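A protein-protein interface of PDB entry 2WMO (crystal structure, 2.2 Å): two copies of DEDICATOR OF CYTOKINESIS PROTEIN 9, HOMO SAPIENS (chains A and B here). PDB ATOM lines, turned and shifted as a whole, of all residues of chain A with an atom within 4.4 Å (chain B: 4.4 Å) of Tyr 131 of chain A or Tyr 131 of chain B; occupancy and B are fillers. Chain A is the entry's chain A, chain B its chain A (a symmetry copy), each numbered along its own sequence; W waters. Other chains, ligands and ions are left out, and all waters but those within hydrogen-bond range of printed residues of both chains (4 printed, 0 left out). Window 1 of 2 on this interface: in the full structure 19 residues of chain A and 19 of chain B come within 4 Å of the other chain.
Of the printed residues of chain B, Ile 115 of chain A touches Lys 112.
Of chain B, only Tyr 131 (3.8 Å), Leu 134 (3.6 Å), His 135 (3.6 Å) and Tyr 138 (3.5 Å) come within 4 Å of Tyr 131 of chain A.
Of the printed residues of chain A, Leu 134 of chain B touches Tyr 131 (3.6 Å).
Of the printed residues of chain A, Tyr 138 of chain B touches Leu 127, Ala 128 and Tyr 131.
The nearest printed residue of chain B that does not touch Tyr 131 of chain A is Ala 108 of chain B (4.1 Å).
The nearest printed residue of chain A that does not touch Tyr 131 of chain B is Ala 108 of chain A (4.1 Å).
The nearest printed residue of chain A that does not touch Leu 134 of chain B is Ala 128 of chain A (5.3 Å).
Water W2 lies within hydrogen-bond range of the side-chain hydroxyl (OH) of Tyr 131 of chain B (2.7 Å) and the side-chain hydroxyl (OH) of Tyr 138 of chain A (2.8 Å).
Water W1 bridges the side-chain hydroxyl of Tyr 131 of chain A (2.7 Å) and the side-chain hydroxyl of Tyr 138 of chain B (2.8 Å).
Water W4 lies within hydrogen-bond range of the side-chain amino group of Lys 112 of chain A and the side-chain hydroxyl of Tyr 131 of chain B.
Water W3 lies within hydrogen-bond range of the side-chain amino group (NZ) of Lys 112 of chain B (3.0 Å) and the side-chain hydroxyl (OH) of Tyr 131 of chain A (3.2 Å).
Hydrophobic or aromatic side chains of chain B within 4 Å of the printed part of chain A: Ile 115, Leu 127, Ala 128, Tyr 131, Leu 134, His 135 and Tyr 138.
Of the 13 printed residues of chain A, 9 touch a printed residue of chain B.
Printed residues of chain A that touch a printed residue of chain B: Lys 112, Ile 115, Leu 127, Ala 128, Tyr 131, Asp 132, Leu 134, His 135 and Tyr 138.
Leu 127 of chain A touches Tyr 138 of chain B, and with the chains exchanged Tyr 138 of chain A touches Leu 127 of chain B.
Ala 128 of chain A touches His 135 of chain B, and with the chains exchanged His 135 of chain A touches Ala 128 of chain B.
Tyr 131 of chain A touches its own counterpart, Tyr 131 of chain B.
Tyr 131 of chain A touches Tyr 138 of chain B, and with the chains exchanged Tyr 138 of chain A touches Tyr 131 of chain B.
13 positions are printed for both chains.
ND1 of His 135 of chain A is in hydrogen-bond range of O of Ala 128 of chain B, at 2.9 Å.
O of Ala 128 of chain A sits at hydrogen-bond distance from ND1 of His 135 of chain B (2.9 Å).
CG2 of Ile 115 of chain B touches NZ of Lys 112 of chain A, 3.5 Å away.
NZ of Lys 112 of chain B touches CG2 of Ile 115 of chain A, at 3.5 Å.
Leu 127 of chain A touches Tyr 138 of chain B (CD1 to CE1, 3.8 Å).
CD1 of Tyr 131 of chain B touches CD1 of Tyr 131 of chain A (3.8 Å).
Tyr 131 of chain A touches Leu 134 of chain B.
Tyr 138 of chain B touches Tyr 131 of chain A.
Asp 132 of chain A touches His 135 of chain B.
ND1 of His 135 of chain A touches CB of Asp 132 of chain B, at 3.4 Å.
N of Ala 128 of chain B touches CB of Tyr 138 of chain A (3.7 Å).
Tyr 138 of chain A touches Tyr 131 of chain B.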
ATOM      1  N   ALA A 108      26.112  -6.107 -12.908  1.00  0.00           N
ATOM      2  CA  ALA A 108      25.688  -5.885 -11.519  1.00  0.00           C
ATOM      3  C   ALA A 108      25.122  -7.150 -10.858  1.00  0.00           C
ATOM      4  O   ALA A 108      25.326  -7.376  -9.668  1.00  0.00           O
ATOM      5  CB  ALA A 108      24.678  -4.689 -11.419  1.00  0.00           C
ATOM      6  N   LYS A 112      26.845  -8.109  -7.332  1.00  0.00           N
ATOM      7  CA  LYS A 112      26.021  -8.154  -6.109  1.00  0.00           C
ATOM      8  C   LYS A 112      26.300  -9.391  -5.260  1.00  0.00           C
ATOM      9  O   LYS A 112      26.092  -9.361  -4.056  1.00  0.00           O
ATOM     10  CB  LYS A 112      24.527  -8.170  -6.443  1.00  0.00           C
ATOM     11  CG  LYS A 112      23.932  -6.875  -6.988  1.00  0.00           C
ATOM     12  CD  LYS A 112      22.436  -7.099  -7.316  1.00  0.00           C
ATOM     13  CE  LYS A 112      21.888  -6.086  -8.327  1.00  0.00           C
ATOM     14  NZ  LYS A 112      22.437  -4.750  -8.092  1.00  0.00           N
ATOM     15  N   ILE A 115      29.959  -8.750  -3.522  1.00  0.00           N
ATOM     16  CA  ILE A 115      30.111  -7.538  -2.718  1.00  0.00           C
ATOM     17  C   ILE A 115      30.100  -7.830  -1.206  1.00  0.00           C
ATOM     18  O   ILE A 115      30.987  -7.391  -0.508  1.00  0.00           O
ATOM     19  CB  ILE A 115      29.116  -6.426  -3.158  1.00  0.00           C
ATOM     20  CG1 ILE A 115      29.660  -5.702  -4.397  1.00  0.00           C
ATOM     21  CG2 ILE A 115      28.814  -5.409  -2.012  1.00  0.00           C
ATOM     22  CD1 ILE A 115      28.603  -4.885  -5.140  1.00  0.00           C
ATOM     23  N   LEU A 127      36.755  -3.828  -3.767  1.00  0.00           N
ATOM     24  CA  LEU A 127      35.492  -3.117  -3.827  1.00  0.00           C
ATOM     25  C   LEU A 127      35.643  -1.912  -4.754  1.00  0.00           C
ATOM     26  O   LEU A 127      34.802  -1.670  -5.602  1.00  0.00           O
ATOM     27  CB  LEU A 127      35.057  -2.694  -2.411  1.00  0.00           C
ATOM     28  CG  LEU A 127      34.484  -3.888  -1.631  1.00  0.00           C
ATOM     29  CD1 LEU A 127      34.392  -3.605  -0.155  1.00  0.00           C
ATOM     30  CD2 LEU A 127      33.102  -4.278  -2.198  1.00  0.00           C
ATOM     31  N   ALA A 128      36.722  -1.156  -4.578  1.00  0.00           N
ATOM     32  CA  ALA A 128      36.973   0.020  -5.411  1.00  0.00           C
ATOM     33  C   ALA A 128      36.965  -0.342  -6.899  1.00  0.00           C
ATOM     34  O   ALA A 128      36.424   0.383  -7.721  1.00  0.00           O
ATOM     35  CB  ALA A 128      38.323   0.657  -5.030  1.00  0.00           C
ATOM     36  N   HIS A 129      37.596  -1.463  -7.222  1.00  0.00           N
ATOM     37  CA  HIS A 129      37.730  -1.914  -8.604  1.00  0.00           C
ATOM     38  C   HIS A 129      36.389  -2.325  -9.203  1.00  0.00           C
ATOM     39  O   HIS A 129      36.050  -1.910 -10.306  1.00  0.00           O
ATOM     40  CB  HIS A 129      38.738  -3.069  -8.709  1.00  0.00           C
ATOM     41  CG  HIS A 129      38.748  -3.733 -10.056  1.00  0.00           C
ATOM     42  ND1 HIS A 129      38.152  -4.955 -10.292  1.00  0.00           N
ATOM     43  CD2 HIS A 129      39.266  -3.333 -11.241  1.00  0.00           C
ATOM     44  CE1 HIS A 129      38.300  -5.277 -11.565  1.00  0.00           C
ATOM     45  NE2 HIS A 129      38.977  -4.310 -12.162  1.00  0.00           N
ATOM     46  N   LEU A 130      35.596  -3.098  -8.471  1.00  0.00           N
ATOM     47  CA  LEU A 130      34.318  -3.522  -9.038  1.00  0.00           C
ATOM     48  C   LEU A 130      33.347  -2.369  -9.226  1.00  0.00           C
ATOM     49  O   LEU A 130      32.648  -2.301 -10.247  1.00  0.00           O
ATOM     50  CB  LEU A 130      33.689  -4.696  -8.277  1.00  0.00           C
ATOM     51  CG  LEU A 130      33.077  -4.568  -6.888  1.00  0.00           C
ATOM     52  CD1 LEU A 130      31.717  -3.833  -6.917  1.00  0.00           C
ATOM     53  CD2 LEU A 130      32.894  -5.971  -6.386  1.00  0.00           C
ATOM     54  N   TYR A 131      33.314  -1.446  -8.265  1.00  0.00           N
ATOM     55  CA  TYR A 131      32.518  -0.233  -8.452  1.00  0.00           C
ATOM     56  C   TYR A 131      33.026   0.607  -9.630  1.00  0.00           C
ATOM     57  O   TYR A 131      32.250   1.233 -10.335  1.00  0.00           O
ATOM     58  CB  TYR A 131      32.456   0.602  -7.155  1.00  0.00           C
ATOM     59  CG  TYR A 131      31.637  -0.077  -6.071  1.00  0.00           C
ATOM     60  CD1 TYR A 131      30.326  -0.463  -6.309  1.00  0.00           C
ATOM     61  CD2 TYR A 131      32.178  -0.342  -4.826  1.00  0.00           C
ATOM     62  CE1 TYR A 131      29.578  -1.084  -5.336  1.00  0.00           C
ATOM     63  CE2 TYR A 131      31.447  -0.973  -3.853  1.00  0.00           C
ATOM     64  CZ  TYR A 131      30.143  -1.331  -4.103  1.00  0.00           C
ATOM     65  OH  TYR A 131      29.407  -1.953  -3.121  1.00  0.00           O
ATOM     66  N   ASP A 132      34.338   0.626  -9.833  1.00  0.00           N
ATOM     67  CA  ASP A 132      34.891   1.282 -11.016  1.00  0.00           C
ATOM     68  C   ASP A 132      34.332   0.644 -12.311  1.00  0.00           C
ATOM     69  O   ASP A 132      33.924   1.340 -13.230  1.00  0.00           O
ATOM     70  CB  ASP A 132      36.416   1.195 -10.987  1.00  0.00           C
ATOM     71  CG  ASP A 132      37.060   1.812 -12.212  1.00  0.00           C
ATOM     72  OD1 ASP A 132      36.576   2.853 -12.698  1.00  0.00           O
ATOM     73  OD2 ASP A 132      38.052   1.238 -12.697  1.00  0.00           O
ATOM     74  N   THR A 133      34.302  -0.682 -12.364  1.00  0.00           N
ATOM     75  CA  THR A 133      33.717  -1.384 -13.508  1.00  0.00           C
ATOM     76  C   THR A 133      32.226  -1.075 -13.649  1.00  0.00           C
ATOM     77  O   THR A 133      31.743  -0.809 -14.767  1.00  0.00           O
ATOM     78  CB  THR A 133      33.938  -2.897 -13.401  1.00  0.00           C
ATOM     79  OG1 THR A 133      35.337  -3.157 -13.425  1.00  0.00           O
ATOM     80  CG2 THR A 133      33.281  -3.646 -14.575  1.00  0.00           C
ATOM     81  N   LEU A 134      31.486  -1.090 -12.536  1.00  0.00           N
ATOM     82  CA  LEU A 134      30.051  -0.814 -12.636  1.00  0.00           C
ATOM     83  C   LEU A 134      29.808   0.600 -13.143  1.00  0.00           C
ATOM     84  O   LEU A 134      28.903   0.836 -13.947  1.00  0.00           O
ATOM     85  CB  LEU A 134      29.331  -1.054 -11.303  1.00  0.00           C
ATOM     86  CG  LEU A 134      29.289  -2.552 -10.960  1.00  0.00           C
ATOM     87  CD1 LEU A 134      28.750  -2.850  -9.533  1.00  0.00           C
ATOM     88  CD2 LEU A 134      28.511  -3.333 -12.056  1.00  0.00           C
ATOM     89  N   HIS A 135      30.615   1.547 -12.677  1.00  0.00           N
ATOM     90  CA  HIS A 135      30.453   2.932 -13.131  1.00  0.00           C
ATOM     91  C   HIS A 135      30.678   3.004 -14.640  1.00  0.00           C
ATOM     92  O   HIS A 135      29.882   3.589 -15.366  1.00  0.00           O
ATOM     93  CB  HIS A 135      31.423   3.883 -12.395  1.00  0.00           C
ATOM     94  CG  HIS A 135      31.605   5.203 -13.080  1.00  0.00           C
ATOM     95  ND1 HIS A 135      30.554   6.056 -13.352  1.00  0.00           N
ATOM     96  CD2 HIS A 135      32.715   5.823 -13.546  1.00  0.00           C
ATOM     97  CE1 HIS A 135      31.006   7.133 -13.963  1.00  0.00           C
ATOM     98  NE2 HIS A 135      32.317   7.019 -14.090  1.00  0.00           N
ATOM     99  N   TYR A 138      27.673   1.331 -16.633  1.00  0.00           N
ATOM    100  CA  TYR A 138      26.468   2.125 -16.838  1.00  0.00           C
ATOM    101  C   TYR A 138      26.708   3.363 -17.720  1.00  0.00           C
ATOM    102  O   TYR A 138      25.810   3.776 -18.459  1.00  0.00           O
ATOM    103  CB  TYR A 138      25.753   2.440 -15.498  1.00  0.00           C
ATOM    104  CG  TYR A 138      25.061   1.199 -14.975  1.00  0.00           C
ATOM    105  CD1 TYR A 138      23.830   0.812 -15.477  1.00  0.00           C
ATOM    106  CD2 TYR A 138      25.671   0.384 -14.041  1.00  0.00           C
ATOM    107  CE1 TYR A 138      23.218  -0.324 -15.043  1.00  0.00           C
ATOM    108  CE2 TYR A 138      25.072  -0.771 -13.608  1.00  0.00           C
ATOM    109  CZ  TYR A 138      23.843  -1.125 -14.118  1.00  0.00           C
ATOM    110  OH  TYR A 138      23.214  -2.274 -13.689  1.00  0.00           O
ATOM    111  N   ALA B 108      27.732   2.615   0.947  1.00  0.00           N
ATOM    112  CA  ALA B 108      27.153   1.446   0.272  1.00  0.00           C
ATOM    113  C   ALA B 108      25.860   0.953   0.935  1.00  0.00           C
ATOM    114  O   ALA B 108      24.942   0.504   0.253  1.00  0.00           O
ATOM    115  CB  ALA B 108      28.204   0.289   0.143  1.00  0.00           C
ATOM    116  N   LYS B 112      22.725   0.578  -1.586  1.00  0.00           N
ATOM    117  CA  LYS B 112      22.102  -0.745  -1.778  1.00  0.00           C
ATOM    118  C   LYS B 112      20.577  -0.686  -1.740  1.00  0.00           C
ATOM    119  O   LYS B 112      19.921  -1.532  -2.330  1.00  0.00           O
ATOM    120  CB  LYS B 112      22.536  -1.731  -0.690  1.00  0.00           C
ATOM    121  CG  LYS B 112      23.978  -2.224  -0.749  1.00  0.00           C
ATOM    122  CD  LYS B 112      24.246  -3.162   0.454  1.00  0.00           C
ATOM    123  CE  LYS B 112      25.735  -3.285   0.795  1.00  0.00           C
ATOM    124  NZ  LYS B 112      26.557  -3.326  -0.416  1.00  0.00           N
ATOM    125  N   ILE B 115      19.440   1.058  -5.275  1.00  0.00           N
ATOM    126  CA  ILE B 115      19.894   0.417  -6.509  1.00  0.00           C
ATOM    127  C   ILE B 115      18.768  -0.365  -7.212  1.00  0.00           C
ATOM    128  O   ILE B 115      18.552  -0.170  -8.388  1.00  0.00           O
ATOM    129  CB  ILE B 115      21.196  -0.404  -6.288  1.00  0.00           C
ATOM    130  CG1 ILE B 115      22.410   0.534  -6.301  1.00  0.00           C
ATOM    131  CG2 ILE B 115      21.368  -1.545  -7.341  1.00  0.00           C
ATOM    132  CD1 ILE B 115      23.671  -0.090  -5.703  1.00  0.00           C
ATOM    133  N   LEU B 127      22.329   5.289 -11.924  1.00  0.00           N
ATOM    134  CA  LEU B 127      23.136   4.147 -11.540  1.00  0.00           C
ATOM    135  C   LEU B 127      24.609   4.478 -11.769  1.00  0.00           C
ATOM    136  O   LEU B 127      25.444   4.229 -10.916  1.00  0.00           O
ATOM    137  CB  LEU B 127      22.702   2.902 -12.336  1.00  0.00           C
ATOM    138  CG  LEU B 127      21.393   2.318 -11.778  1.00  0.00           C
ATOM    139  CD1 LEU B 127      20.756   1.346 -12.734  1.00  0.00           C
ATOM    140  CD2 LEU B 127      21.653   1.648 -10.412  1.00  0.00           C
ATOM    141  N   ALA B 128      24.920   5.035 -12.935  1.00  0.00           N
ATOM    142  CA  ALA B 128      26.299   5.399 -13.262  1.00  0.00           C
ATOM    143  C   ALA B 128      26.898   6.320 -12.195  1.00  0.00           C
ATOM    144  O   ALA B 128      28.047   6.170 -11.805  1.00  0.00           O
ATOM    145  CB  ALA B 128      26.350   6.086 -14.640  1.00  0.00           C
ATOM    146  N   HIS B 129      26.102   7.285 -11.754  1.00  0.00           N
ATOM    147  CA  HIS B 129      26.544   8.280 -10.782  1.00  0.00           C
ATOM    148  C   HIS B 129      26.798   7.665  -9.410  1.00  0.00           C
ATOM    149  O   HIS B 129      27.836   7.910  -8.805  1.00  0.00           O
ATOM    150  CB  HIS B 129      25.528   9.428 -10.672  1.00  0.00           C
ATOM    151  CG  HIS B 129      25.803  10.361  -9.527  1.00  0.00           C
ATOM    152  ND1 HIS B 129      25.080  10.337  -8.352  1.00  0.00           N
ATOM    153  CD2 HIS B 129      26.734  11.332  -9.374  1.00  0.00           C
ATOM    154  CE1 HIS B 129      25.557  11.249  -7.524  1.00  0.00           C
ATOM    155  NE2 HIS B 129      26.559  11.870  -8.123  1.00  0.00           N
ATOM    156  N   LEU B 130      25.888   6.828  -8.929  1.00  0.00           N
ATOM    157  CA  LEU B 130      26.103   6.247  -7.606  1.00  0.00           C
ATOM    158  C   LEU B 130      27.286   5.294  -7.568  1.00  0.00           C
ATOM    159  O   LEU B 130      28.061   5.298  -6.601  1.00  0.00           O
ATOM    160  CB  LEU B 130      24.832   5.625  -7.014  1.00  0.00           C
ATOM    161  CG  LEU B 130      24.211   4.332  -7.525  1.00  0.00           C
ATOM    162  CD1 LEU B 130      25.034   3.089  -7.113  1.00  0.00           C
ATOM    163  CD2 LEU B 130      22.839   4.265  -6.920  1.00  0.00           C
ATOM    164  N   TYR B 131      27.447   4.492  -8.620  1.00  0.00           N
ATOM    165  CA  TYR B 131      28.647   3.661  -8.721  1.00  0.00           C
ATOM    166  C   TYR B 131      29.922   4.506  -8.812  1.00  0.00           C
ATOM    167  O   TYR B 131      30.963   4.131  -8.296  1.00  0.00           O
ATOM    168  CB  TYR B 131      28.545   2.671  -9.901  1.00  0.00           C
ATOM    169  CG  TYR B 131      27.504   1.591  -9.661  1.00  0.00           C
ATOM    170  CD1 TYR B 131      27.560   0.791  -8.529  1.00  0.00           C
ATOM    171  CD2 TYR B 131      26.466   1.387 -10.552  1.00  0.00           C
ATOM    172  CE1 TYR B 131      26.619  -0.185  -8.299  1.00  0.00           C
ATOM    173  CE2 TYR B 131      25.514   0.428 -10.327  1.00  0.00           C
ATOM    174  CZ  TYR B 131      25.598  -0.367  -9.209  1.00  0.00           C
ATOM    175  OH  TYR B 131      24.648  -1.339  -8.990  1.00  0.00           O
ATOM    176  N   ASP B 132      29.839   5.649  -9.484  1.00  0.00           N
ATOM    177  CA  ASP B 132      30.966   6.580  -9.496  1.00  0.00           C
ATOM    178  C   ASP B 132      31.324   7.029  -8.059  1.00  0.00           C
ATOM    179  O   ASP B 132      32.485   7.045  -7.677  1.00  0.00           O
ATOM    180  CB  ASP B 132      30.625   7.787 -10.369  1.00  0.00           C
ATOM    181  CG  ASP B 132      31.731   8.823 -10.389  1.00  0.00           C
ATOM    182  OD1 ASP B 132      32.919   8.449 -10.406  1.00  0.00           O
ATOM    183  OD2 ASP B 132      31.401  10.023 -10.376  1.00  0.00           O
ATOM    184  N   THR B 133      30.316   7.374  -7.267  1.00  0.00           N
ATOM    185  CA  THR B 133      30.540   7.734  -5.866  1.00  0.00           C
ATOM    186  C   THR B 133      31.116   6.560  -5.073  1.00  0.00           C
ATOM    187  O   THR B 133      32.069   6.738  -4.290  1.00  0.00           O
ATOM    188  CB  THR B 133      29.248   8.235  -5.210  1.00  0.00           C
ATOM    189  OG1 THR B 133      28.824   9.417  -5.881  1.00  0.00           O
ATOM    190  CG2 THR B 133      29.464   8.567  -3.723  1.00  0.00           C
ATOM    191  N   LEU B 134      30.566   5.357  -5.268  1.00  0.00           N
ATOM    192  CA  LEU B 134      31.082   4.212  -4.515  1.00  0.00           C
ATOM    193  C   LEU B 134      32.538   3.944  -4.870  1.00  0.00           C
ATOM    194  O   LEU B 134      33.351   3.621  -4.001  1.00  0.00           O
ATOM    195  CB  LEU B 134      30.222   2.959  -4.723  1.00  0.00           C
ATOM    196  CG  LEU B 134      28.846   3.117  -4.056  1.00  0.00           C
ATOM    197  CD1 LEU B 134      27.855   1.968  -4.394  1.00  0.00           C
ATOM    198  CD2 LEU B 134      29.011   3.317  -2.524  1.00  0.00           C
ATOM    199  N   HIS B 135      32.873   4.075  -6.149  1.00  0.00           N
ATOM    200  CA  HIS B 135      34.259   3.849  -6.568  1.00  0.00           C
ATOM    201  C   HIS B 135      35.173   4.853  -5.869  1.00  0.00           C
ATOM    202  O   HIS B 135      36.198   4.484  -5.306  1.00  0.00           O
ATOM    203  CB  HIS B 135      34.410   3.957  -8.101  1.00  0.00           C
ATOM    204  CG  HIS B 135      35.826   4.147  -8.554  1.00  0.00           C
ATOM    205  ND1 HIS B 135      36.835   3.254  -8.251  1.00  0.00           N
ATOM    206  CD2 HIS B 135      36.405   5.124  -9.290  1.00  0.00           C
ATOM    207  CE1 HIS B 135      37.969   3.677  -8.770  1.00  0.00           C
ATOM    208  NE2 HIS B 135      37.736   4.810  -9.411  1.00  0.00           N
ATOM    209  N   TYR B 138      35.539   4.032  -1.997  1.00  0.00           N
ATOM    210  CA  TYR B 138      36.488   2.995  -1.609  1.00  0.00           C
ATOM    211  C   TYR B 138      37.945   3.362  -1.936  1.00  0.00           C
ATOM    212  O   TYR B 138      38.859   2.964  -1.209  1.00  0.00           O
ATOM    213  CB  TYR B 138      36.060   1.600  -2.136  1.00  0.00           C
ATOM    214  CG  TYR B 138      34.888   1.079  -1.332  1.00  0.00           C
ATOM    215  CD1 TYR B 138      35.086   0.490  -0.094  1.00  0.00           C
ATOM    216  CD2 TYR B 138      33.590   1.244  -1.776  1.00  0.00           C
ATOM    217  CE1 TYR B 138      34.035   0.055   0.655  1.00  0.00           C
ATOM    218  CE2 TYR B 138      32.523   0.825  -1.024  1.00  0.00           C
ATOM    219  CZ  TYR B 138      32.752   0.233   0.199  1.00  0.00           C
ATOM    220  OH  TYR B 138      31.697  -0.209   0.968  1.00  0.00           O
HETATM  221  O   HOH W   1      30.342  -2.084  -0.608  1.00  0.00           O
HETATM  222  O   HOH W   2      22.899  -1.978 -10.923  1.00  0.00           O
HETATM  223  O   HOH W   3      26.257  -2.453  -3.238  1.00  0.00           O
HETATM  224  O   HOH W   4      24.849  -3.626  -6.774  1.00  0.00           O
